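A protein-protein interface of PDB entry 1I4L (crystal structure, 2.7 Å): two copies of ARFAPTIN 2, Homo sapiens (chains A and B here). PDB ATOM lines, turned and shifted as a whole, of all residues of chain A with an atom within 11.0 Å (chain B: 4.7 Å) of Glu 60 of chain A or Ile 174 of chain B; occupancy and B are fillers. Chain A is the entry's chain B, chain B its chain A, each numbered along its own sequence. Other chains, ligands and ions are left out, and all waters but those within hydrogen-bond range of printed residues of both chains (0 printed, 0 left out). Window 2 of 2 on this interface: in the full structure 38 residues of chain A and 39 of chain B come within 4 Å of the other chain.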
ATOM      1  N   PHE A  51       7.269   9.061 -12.487  1.00  0.00           N
ATOM      2  CA  PHE A  51       6.741  10.287 -13.094  1.00  0.00           C
ATOM      3  C   PHE A  51       5.245  10.481 -12.814  1.00  0.00           C
ATOM      4  O   PHE A  51       4.784  11.607 -12.609  1.00  0.00           O
ATOM      5  CB  PHE A  51       6.982  10.294 -14.613  1.00  0.00           C
ATOM      6  CG  PHE A  51       8.410  10.516 -15.013  1.00  0.00           C
ATOM      7  CD1 PHE A  51       8.885  10.012 -16.217  1.00  0.00           C
ATOM      8  CD2 PHE A  51       9.270  11.252 -14.215  1.00  0.00           C
ATOM      9  CE1 PHE A  51      10.196  10.237 -16.623  1.00  0.00           C
ATOM     10  CE2 PHE A  51      10.589  11.486 -14.609  1.00  0.00           C
ATOM     11  CZ  PHE A  51      11.051  10.976 -15.816  1.00  0.00           C
ATOM     12  N   ASP A  53       3.651   9.496 -10.194  1.00  0.00           N
ATOM     13  CA  ASP A  53       3.614   9.925  -8.820  1.00  0.00           C
ATOM     14  C   ASP A  53       3.951  11.411  -8.673  1.00  0.00           C
ATOM     15  O   ASP A  53       3.217  12.153  -8.026  1.00  0.00           O
ATOM     16  CB  ASP A  53       4.580   9.080  -7.996  1.00  0.00           C
ATOM     17  CG  ASP A  53       4.792   9.642  -6.610  1.00  0.00           C
ATOM     18  OD1 ASP A  53       3.786   9.903  -5.908  1.00  0.00           O
ATOM     19  OD2 ASP A  53       5.970   9.828  -6.231  1.00  0.00           O
ATOM     20  N   LEU A  54       5.067  11.837  -9.261  1.00  0.00           N
ATOM     21  CA  LEU A  54       5.481  13.225  -9.181  1.00  0.00           C
ATOM     22  C   LEU A  54       4.411  14.109  -9.788  1.00  0.00           C
ATOM     23  O   LEU A  54       4.184  15.229  -9.343  1.00  0.00           O
ATOM     24  CB  LEU A  54       6.797  13.429  -9.920  1.00  0.00           C
ATOM     25  CG  LEU A  54       8.110  13.701  -9.171  1.00  0.00           C
ATOM     26  CD1 LEU A  54       7.801  14.131  -7.764  1.00  0.00           C
ATOM     27  CD2 LEU A  54       9.001  12.480  -9.185  1.00  0.00           C
ATOM     28  N   SER A  55       3.740  13.599 -10.808  1.00  0.00           N
ATOM     29  CA  SER A  55       2.686  14.364 -11.462  1.00  0.00           C
ATOM     30  C   SER A  55       1.566  14.671 -10.479  1.00  0.00           C
ATOM     31  O   SER A  55       1.071  15.789 -10.430  1.00  0.00           O
ATOM     32  CB  SER A  55       2.121  13.596 -12.659  1.00  0.00           C
ATOM     33  OG  SER A  55       1.171  14.392 -13.343  1.00  0.00           O
ATOM     34  N   GLN A  56       1.169  13.669  -9.701  1.00  0.00           N
ATOM     35  CA  GLN A  56       0.109  13.838  -8.712  1.00  0.00           C
ATOM     36  C   GLN A  56       0.506  14.760  -7.570  1.00  0.00           C
ATOM     37  O   GLN A  56      -0.321  15.492  -7.043  1.00  0.00           O
ATOM     38  CB  GLN A  56      -0.299  12.481  -8.150  1.00  0.00           C
ATOM     39  CG  GLN A  56      -1.309  11.765  -9.021  1.00  0.00           C
ATOM     40  CD  GLN A  56      -1.357  10.272  -8.770  1.00  0.00           C
ATOM     41  OE1 GLN A  56      -1.387   9.822  -7.621  1.00  0.00           O
ATOM     42  NE2 GLN A  56      -1.378   9.491  -9.851  1.00  0.00           N
ATOM     43  N   LYS A  57       1.779  14.735  -7.200  1.00  0.00           N
ATOM     44  CA  LYS A  57       2.267  15.559  -6.109  1.00  0.00           C
ATOM     45  C   LYS A  57       2.779  16.944  -6.488  1.00  0.00           C
ATOM     46  O   LYS A  57       2.712  17.872  -5.676  1.00  0.00           O
ATOM     47  CB  LYS A  57       3.355  14.802  -5.352  1.00  0.00           C
ATOM     48  CG  LYS A  57       2.858  14.156  -4.068  1.00  0.00           C
ATOM     49  CD  LYS A  57       1.620  13.288  -4.268  1.00  0.00           C
ATOM     50  CE  LYS A  57       1.979  11.880  -4.702  1.00  0.00           C
ATOM     51  NZ  LYS A  57       0.760  11.019  -4.847  1.00  0.00           N
ATOM     52  N   SER A  58       3.281  17.100  -7.709  1.00  0.00           N
ATOM     53  CA  SER A  58       3.815  18.391  -8.127  1.00  0.00           C
ATOM     54  C   SER A  58       2.896  19.189  -9.041  1.00  0.00           C
ATOM     55  O   SER A  58       3.121  19.270 -10.244  1.00  0.00           O
ATOM     56  CB  SER A  58       5.152  18.197  -8.827  1.00  0.00           C
ATOM     57  OG  SER A  58       5.905  17.193  -8.186  1.00  0.00           O
ATOM     58  N   PRO A  59       1.851  19.808  -8.483  1.00  0.00           N
ATOM     59  CA  PRO A  59       0.971  20.580  -9.361  1.00  0.00           C
ATOM     60  C   PRO A  59       1.699  21.627 -10.235  1.00  0.00           C
ATOM     61  O   PRO A  59       1.211  21.983 -11.309  1.00  0.00           O
ATOM     62  CB  PRO A  59      -0.041  21.192  -8.378  1.00  0.00           C
ATOM     63  CG  PRO A  59       0.716  21.254  -7.088  1.00  0.00           C
ATOM     64  CD  PRO A  59       1.441  19.939  -7.076  1.00  0.00           C
ATOM     65  N   GLU A  60       2.861  22.109  -9.792  1.00  0.00           N
ATOM     66  CA  GLU A  60       3.611  23.095 -10.586  1.00  0.00           C
ATOM     67  C   GLU A  60       4.190  22.467 -11.859  1.00  0.00           C
ATOM     68  O   GLU A  60       4.453  23.160 -12.839  1.00  0.00           O
ATOM     69  CB  GLU A  60       4.782  23.697  -9.799  1.00  0.00           C
ATOM     70  CG  GLU A  60       4.742  23.494  -8.312  1.00  0.00           C
ATOM     71  CD  GLU A  60       5.056  22.070  -7.899  1.00  0.00           C
ATOM     72  OE1 GLU A  60       6.246  21.683  -7.934  1.00  0.00           O
ATOM     73  OE2 GLU A  60       4.105  21.339  -7.539  1.00  0.00           O
ATOM     74  N   LEU A  61       4.389  21.156 -11.829  1.00  0.00           N
ATOM     75  CA  LEU A  61       4.956  20.428 -12.949  1.00  0.00           C
ATOM     76  C   LEU A  61       4.093  19.216 -13.242  1.00  0.00           C
ATOM     77  O   LEU A  61       4.591  18.154 -13.591  1.00  0.00           O
ATOM     78  CB  LEU A  61       6.368  19.991 -12.580  1.00  0.00           C
ATOM     79  CG  LEU A  61       7.330  21.157 -12.313  1.00  0.00           C
ATOM     80  CD1 LEU A  61       8.481  20.682 -11.463  1.00  0.00           C
ATOM     81  CD2 LEU A  61       7.850  21.721 -13.621  1.00  0.00           C
ATOM     82  N   GLN A  62       2.787  19.389 -13.112  1.00  0.00           N
ATOM     83  CA  GLN A  62       1.849  18.298 -13.317  1.00  0.00           C
ATOM     84  C   GLN A  62       1.798  17.752 -14.727  1.00  0.00           C
ATOM     85  O   GLN A  62       1.798  16.538 -14.918  1.00  0.00           O
ATOM     86  CB  GLN A  62       0.454  18.740 -12.893  1.00  0.00           C
ATOM     87  CG  GLN A  62      -0.613  17.690 -13.118  1.00  0.00           C
ATOM     88  CD  GLN A  62      -1.973  18.098 -12.565  1.00  0.00           C
ATOM     89  OE1 GLN A  62      -2.961  17.380 -12.737  1.00  0.00           O
ATOM     90  NE2 GLN A  62      -2.027  19.250 -11.888  1.00  0.00           N
ATOM     91  N   GLU A  63       1.735  18.649 -15.708  1.00  0.00           N
ATOM     92  CA  GLU A  63       1.674  18.255 -17.114  1.00  0.00           C
ATOM     93  C   GLU A  63       2.962  17.601 -17.577  1.00  0.00           C
ATOM     94  O   GLU A  63       2.939  16.528 -18.173  1.00  0.00           O
ATOM     95  CB  GLU A  63       1.428  19.468 -18.003  1.00  0.00           C
ATOM     96  CG  GLU A  63       0.051  20.075 -17.949  1.00  0.00           C
ATOM     97  CD  GLU A  63      -0.091  21.180 -18.988  1.00  0.00           C
ATOM     98  OE1 GLU A  63       0.686  22.166 -18.918  1.00  0.00           O
ATOM     99  OE2 GLU A  63      -0.966  21.055 -19.878  1.00  0.00           O
ATOM    100  N   GLU A  64       4.077  18.276 -17.318  1.00  0.00           N
ATOM    101  CA  GLU A  64       5.390  17.795 -17.696  1.00  0.00           C
ATOM    102  C   GLU A  64       5.657  16.396 -17.147  1.00  0.00           C
ATOM    103  O   GLU A  64       6.159  15.530 -17.862  1.00  0.00           O
ATOM    104  CB  GLU A  64       6.465  18.767 -17.209  1.00  0.00           C
ATOM    105  CG  GLU A  64       6.304  20.185 -17.719  1.00  0.00           C
ATOM    106  CD  GLU A  64       5.363  21.004 -16.865  1.00  0.00           C
ATOM    107  OE1 GLU A  64       4.362  20.446 -16.382  1.00  0.00           O
ATOM    108  OE2 GLU A  64       5.612  22.213 -16.677  1.00  0.00           O
ATOM    109  N   PHE A  65       5.335  16.160 -15.880  1.00  0.00           N
ATOM    110  CA  PHE A  65       5.536  14.826 -15.333  1.00  0.00           C
ATOM    111  C   PHE A  65       4.454  13.916 -15.917  1.00  0.00           C
ATOM    112  O   PHE A  65       4.668  12.719 -16.110  1.00  0.00           O
ATOM    113  CB  PHE A  65       5.476  14.845 -13.792  1.00  0.00           C
ATOM    114  CG  PHE A  65       6.776  15.255 -13.122  1.00  0.00           C
ATOM    115  CD1 PHE A  65       6.831  16.382 -12.299  1.00  0.00           C
ATOM    116  CD2 PHE A  65       7.921  14.501 -13.281  1.00  0.00           C
ATOM    117  CE1 PHE A  65       7.999  16.747 -11.644  1.00  0.00           C
ATOM    118  CE2 PHE A  65       9.107  14.854 -12.624  1.00  0.00           C
ATOM    119  CZ  PHE A  65       9.142  15.983 -11.803  1.00  0.00           C
ATOM    120  N   GLY A  66       3.300  14.506 -16.217  1.00  0.00           N
ATOM    121  CA  GLY A  66       2.187  13.768 -16.789  1.00  0.00           C
ATOM    122  C   GLY A  66       2.444  13.185 -18.170  1.00  0.00           C
ATOM    123  O   GLY A  66       2.319  11.961 -18.374  1.00  0.00           O
ATOM    124  N   TYR A  67       2.814  14.020 -19.142  1.00  0.00           N
ATOM    125  CA  TYR A  67       3.052  13.445 -20.455  1.00  0.00           C
ATOM    126  C   TYR A  67       4.267  12.547 -20.466  1.00  0.00           C
ATOM    127  O   TYR A  67       4.337  11.621 -21.269  1.00  0.00           O
ATOM    128  CB  TYR A  67       3.117  14.509 -21.570  1.00  0.00           C
ATOM    129  CG  TYR A  67       4.072  15.672 -21.420  1.00  0.00           C
ATOM    130  CD1 TYR A  67       5.456  15.496 -21.538  1.00  0.00           C
ATOM    131  CD2 TYR A  67       3.586  16.969 -21.220  1.00  0.00           C
ATOM    132  CE1 TYR A  67       6.335  16.593 -21.464  1.00  0.00           C
ATOM    133  CE2 TYR A  67       4.451  18.061 -21.141  1.00  0.00           C
ATOM    134  CZ  TYR A  67       5.823  17.868 -21.265  1.00  0.00           C
ATOM    135  OH  TYR A  67       6.670  18.953 -21.194  1.00  0.00           O
ATOM    136  N   GLU B 170      12.246  26.918  -5.049  1.00  0.00           N
ATOM    137  CA  GLU B 170      11.053  26.445  -5.719  1.00  0.00           C
ATOM    138  C   GLU B 170      10.947  27.050  -7.121  1.00  0.00           C
ATOM    139  O   GLU B 170      10.570  26.362  -8.069  1.00  0.00           O
ATOM    140  CB  GLU B 170       9.808  26.798  -4.921  1.00  0.00           C
ATOM    141  CG  GLU B 170       8.523  26.342  -5.597  1.00  0.00           C
ATOM    142  CD  GLU B 170       8.377  24.825  -5.655  1.00  0.00           C
ATOM    143  OE1 GLU B 170       9.253  24.098  -5.115  1.00  0.00           O
ATOM    144  OE2 GLU B 170       7.371  24.355  -6.239  1.00  0.00           O
ATOM    145  N   GLU B 171      11.283  28.339  -7.234  1.00  0.00           N
ATOM    146  CA  GLU B 171      11.242  29.072  -8.495  1.00  0.00           C
ATOM    147  C   GLU B 171      12.177  28.431  -9.495  1.00  0.00           C
ATOM    148  O   GLU B 171      11.793  28.143 -10.634  1.00  0.00           O
ATOM    149  CB  GLU B 171      11.661  30.528  -8.282  1.00  0.00           C
ATOM    150  CG  GLU B 171      10.544  31.460  -7.830  1.00  0.00           C
ATOM    151  CD  GLU B 171      11.067  32.794  -7.297  1.00  0.00           C
ATOM    152  OE1 GLU B 171      12.052  33.320  -7.873  1.00  0.00           O
ATOM    153  OE2 GLU B 171      10.494  33.320  -6.311  1.00  0.00           O
ATOM    154  N   ASN B 172      13.412  28.209  -9.065  1.00  0.00           N
ATOM    155  CA  ASN B 172      14.394  27.586  -9.923  1.00  0.00           C
ATOM    156  C   ASN B 172      14.063  26.124 -10.254  1.00  0.00           C
ATOM    157  O   ASN B 172      14.378  25.650 -11.344  1.00  0.00           O
ATOM    158  CB  ASN B 172      15.771  27.699  -9.271  1.00  0.00           C
ATOM    159  CG  ASN B 172      16.737  28.510 -10.111  1.00  0.00           C
ATOM    160  OD1 ASN B 172      17.474  27.956 -10.936  1.00  0.00           O
ATOM    161  ND2 ASN B 172      16.718  29.838  -9.932  1.00  0.00           N
ATOM    162  N   LYS B 173      13.421  25.419  -9.324  1.00  0.00           N
ATOM    163  CA  LYS B 173      13.059  24.023  -9.533  1.00  0.00           C
ATOM    164  C   LYS B 173      12.047  23.895 -10.672  1.00  0.00           C
ATOM    165  O   LYS B 173      12.141  22.998 -11.503  1.00  0.00           O
ATOM    166  CB  LYS B 173      12.470  23.421  -8.251  1.00  0.00           C
ATOM    167  CG  LYS B 173      12.160  21.936  -8.362  1.00  0.00           C
ATOM    168  CD  LYS B 173      11.157  21.487  -7.329  1.00  0.00           C
ATOM    169  CE  LYS B 173       9.816  22.120  -7.572  1.00  0.00           C
ATOM    170  NZ  LYS B 173       8.795  21.717  -6.576  1.00  0.00           N
ATOM    171  N   ILE B 174      11.074  24.796 -10.713  1.00  0.00           N
ATOM    172  CA  ILE B 174      10.077  24.764 -11.776  1.00  0.00           C
ATOM    173  C   ILE B 174      10.756  24.947 -13.140  1.00  0.00           C
ATOM    174  O   ILE B 174      10.506  24.186 -14.076  1.00  0.00           O
ATOM    175  CB  ILE B 174       9.053  25.894 -11.613  1.00  0.00           C
ATOM    176  CG1 ILE B 174       8.643  26.015 -10.142  1.00  0.00           C
ATOM    177  CG2 ILE B 174       7.871  25.637 -12.521  1.00  0.00           C
ATOM    178  CD1 ILE B 174       7.232  25.630  -9.829  1.00  0.00           C
ATOM    179  N   LYS B 175      11.615  25.963 -13.240  1.00  0.00           N
ATOM    180  CA  LYS B 175      12.325  26.265 -14.479  1.00  0.00           C
ATOM    181  C   LYS B 175      13.194  25.128 -14.980  1.00  0.00           C
ATOM    182  O   LYS B 175      13.061  24.702 -16.132  1.00  0.00           O
ATOM    183  CB  LYS B 175      13.167  27.530 -14.317  1.00  0.00           C
ATOM    184  CG  LYS B 175      12.332  28.789 -14.364  1.00  0.00           C
ATOM    185  CD  LYS B 175      13.047  29.977 -13.752  1.00  0.00           C
ATOM    186  CE  LYS B 175      12.064  31.132 -13.530  1.00  0.00           C
ATOM    187  NZ  LYS B 175      12.718  32.314 -12.889  1.00  0.00           N
ATOM    188  N   VAL B 176      14.081  24.641 -14.124  1.00  0.00           N
ATOM    189  CA  VAL B 176      14.952  23.545 -14.503  1.00  0.00           C
ATOM    190  C   VAL B 176      14.175  22.292 -14.931  1.00  0.00           C
ATOM    191  O   VAL B 176      14.475  21.688 -15.966  1.00  0.00           O
ATOM    192  CB  VAL B 176      15.886  23.148 -13.337  1.00  0.00           C
ATOM    193  CG1 VAL B 176      16.723  21.931 -13.721  1.00  0.00           C
ATOM    194  CG2 VAL B 176      16.756  24.311 -12.956  1.00  0.00           C
ATOM    195  N   MET B 177      13.181  21.904 -14.131  1.00  0.00           N
ATOM    196  CA  MET B 177      12.404  20.705 -14.423  1.00  0.00           C
ATOM    197  C   MET B 177      11.528  20.862 -15.638  1.00  0.00           C
ATOM    198  O   MET B 177      11.334  19.920 -16.404  1.00  0.00           O
ATOM    199  CB  MET B 177      11.531  20.303 -13.217  1.00  0.00           C
ATOM    200  CG  MET B 177      12.305  19.837 -12.028  1.00  0.00           C
ATOM    201  SD  MET B 177      13.517  18.623 -12.521  1.00  0.00           S
ATOM    202  CE  MET B 177      12.573  17.116 -12.348  1.00  0.00           C
ATOM    203  N   HIS B 178      10.961  22.042 -15.806  1.00  0.00           N
ATOM    204  CA  HIS B 178      10.125  22.263 -16.968  1.00  0.00           C
ATOM    205  C   HIS B 178      10.957  22.048 -18.233  1.00  0.00           C
ATOM    206  O   HIS B 178      10.617  21.222 -19.095  1.00  0.00           O
ATOM    207  CB  HIS B 178       9.578  23.667 -16.959  1.00  0.00           C
ATOM    208  CG  HIS B 178       8.777  23.987 -18.174  1.00  0.00           C
ATOM    209  ND1 HIS B 178       9.228  24.842 -19.158  1.00  0.00           N
ATOM    210  CD2 HIS B 178       7.562  23.549 -18.576  1.00  0.00           C
ATOM    211  CE1 HIS B 178       8.320  24.918 -20.113  1.00  0.00           C
ATOM    212  NE2 HIS B 178       7.301  24.142 -19.785  1.00  0.00           N
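The side-chain carboxylate of Glu 60 of chain A is in salt-bridge range of the side-chain amino group of Lys 173 of chain B (2.9 Å).
OE1 of Glu 60 of chain A lies close to OE2 of Glu 170 of chain B (3.4 Å).
The side-chain amino group (NZ) of Lys 173 of chain B is in salt-bridge range of the side-chain carboxylate (OE1) of Glu 170 of chain B.
Among the printed residues, merely in contact across the chains: Glu 64 of chain A with His 178 of chain B (3.0 Å), Glu 60 of chain A with Ile 174 of chain B (3.1 Å), Leu 61 of chain A with Met 177 of chain B (3.5 Å), Leu 61 of chain A with Ile 174 of chain B (3.7 Å), Phe 65 of chain A with Met 177 of chain B (3.7 Å) and Leu 61 of chain A with His 178 of chain B (3.8 Å).
Phe 51 of chain A touches none of the printed residues of chain B.
Of the printed residues of chain B, Leu 61 of chain A touches Ile 174 (3.7 Å), Met 177 (3.5 Å) and His 178 (3.8 Å).
Gln 62 of chain A touches none of the printed residues of chain B.
Of the printed residues of chain B, Glu 64 of chain A touches His 178 (3.0 Å).
Printed residues of chain B within 4 Å of Phe 65 of chain A: Met 177.
Of the printed residues of chain A, Glu 170 of chain B touches Glu 60 (3.4 Å).
Of chain A, only Glu 60 and Leu 61 come within 4 Å of Ile 174 of chain B.
No residue of chain A comes within 4 Å of Val 176 of chain B.
Printed residues of chain A within 4 Å of Met 177 of chain B: Leu 61 and Phe 65.
Of chain A, only Leu 61 (3.8 Å) and Glu 64 (3.0 Å) come within 4 Å of His 178 of chain B.
The nearest printed residue of chain B that does not touch Glu 60 of chain A is His 178 of chain B (6.5 Å).
Hydrophobic or aromatic side chains of chain A within 4 Å of the printed part of chain B: Leu 61 and Phe 65.
Of the 9 printed residues of chain B, 5 touch a printed residue of chain A.
Hydrophobic or aromatic side chains of chain B within 4 Å of the printed part of chain A: Ile 174, Met 177 and His 178.
Among the printed residues, Asp or Glu carboxylates within 4 Å of a Lys or Arg side-chain nitrogen of the other chain: Glu 60 of chain A with Lys 173 of chain B.
No position is printed for both chains.
Of the 8 pairs that touch across the chains among the printed residues, none has its exchanged pair printed and touching as well.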
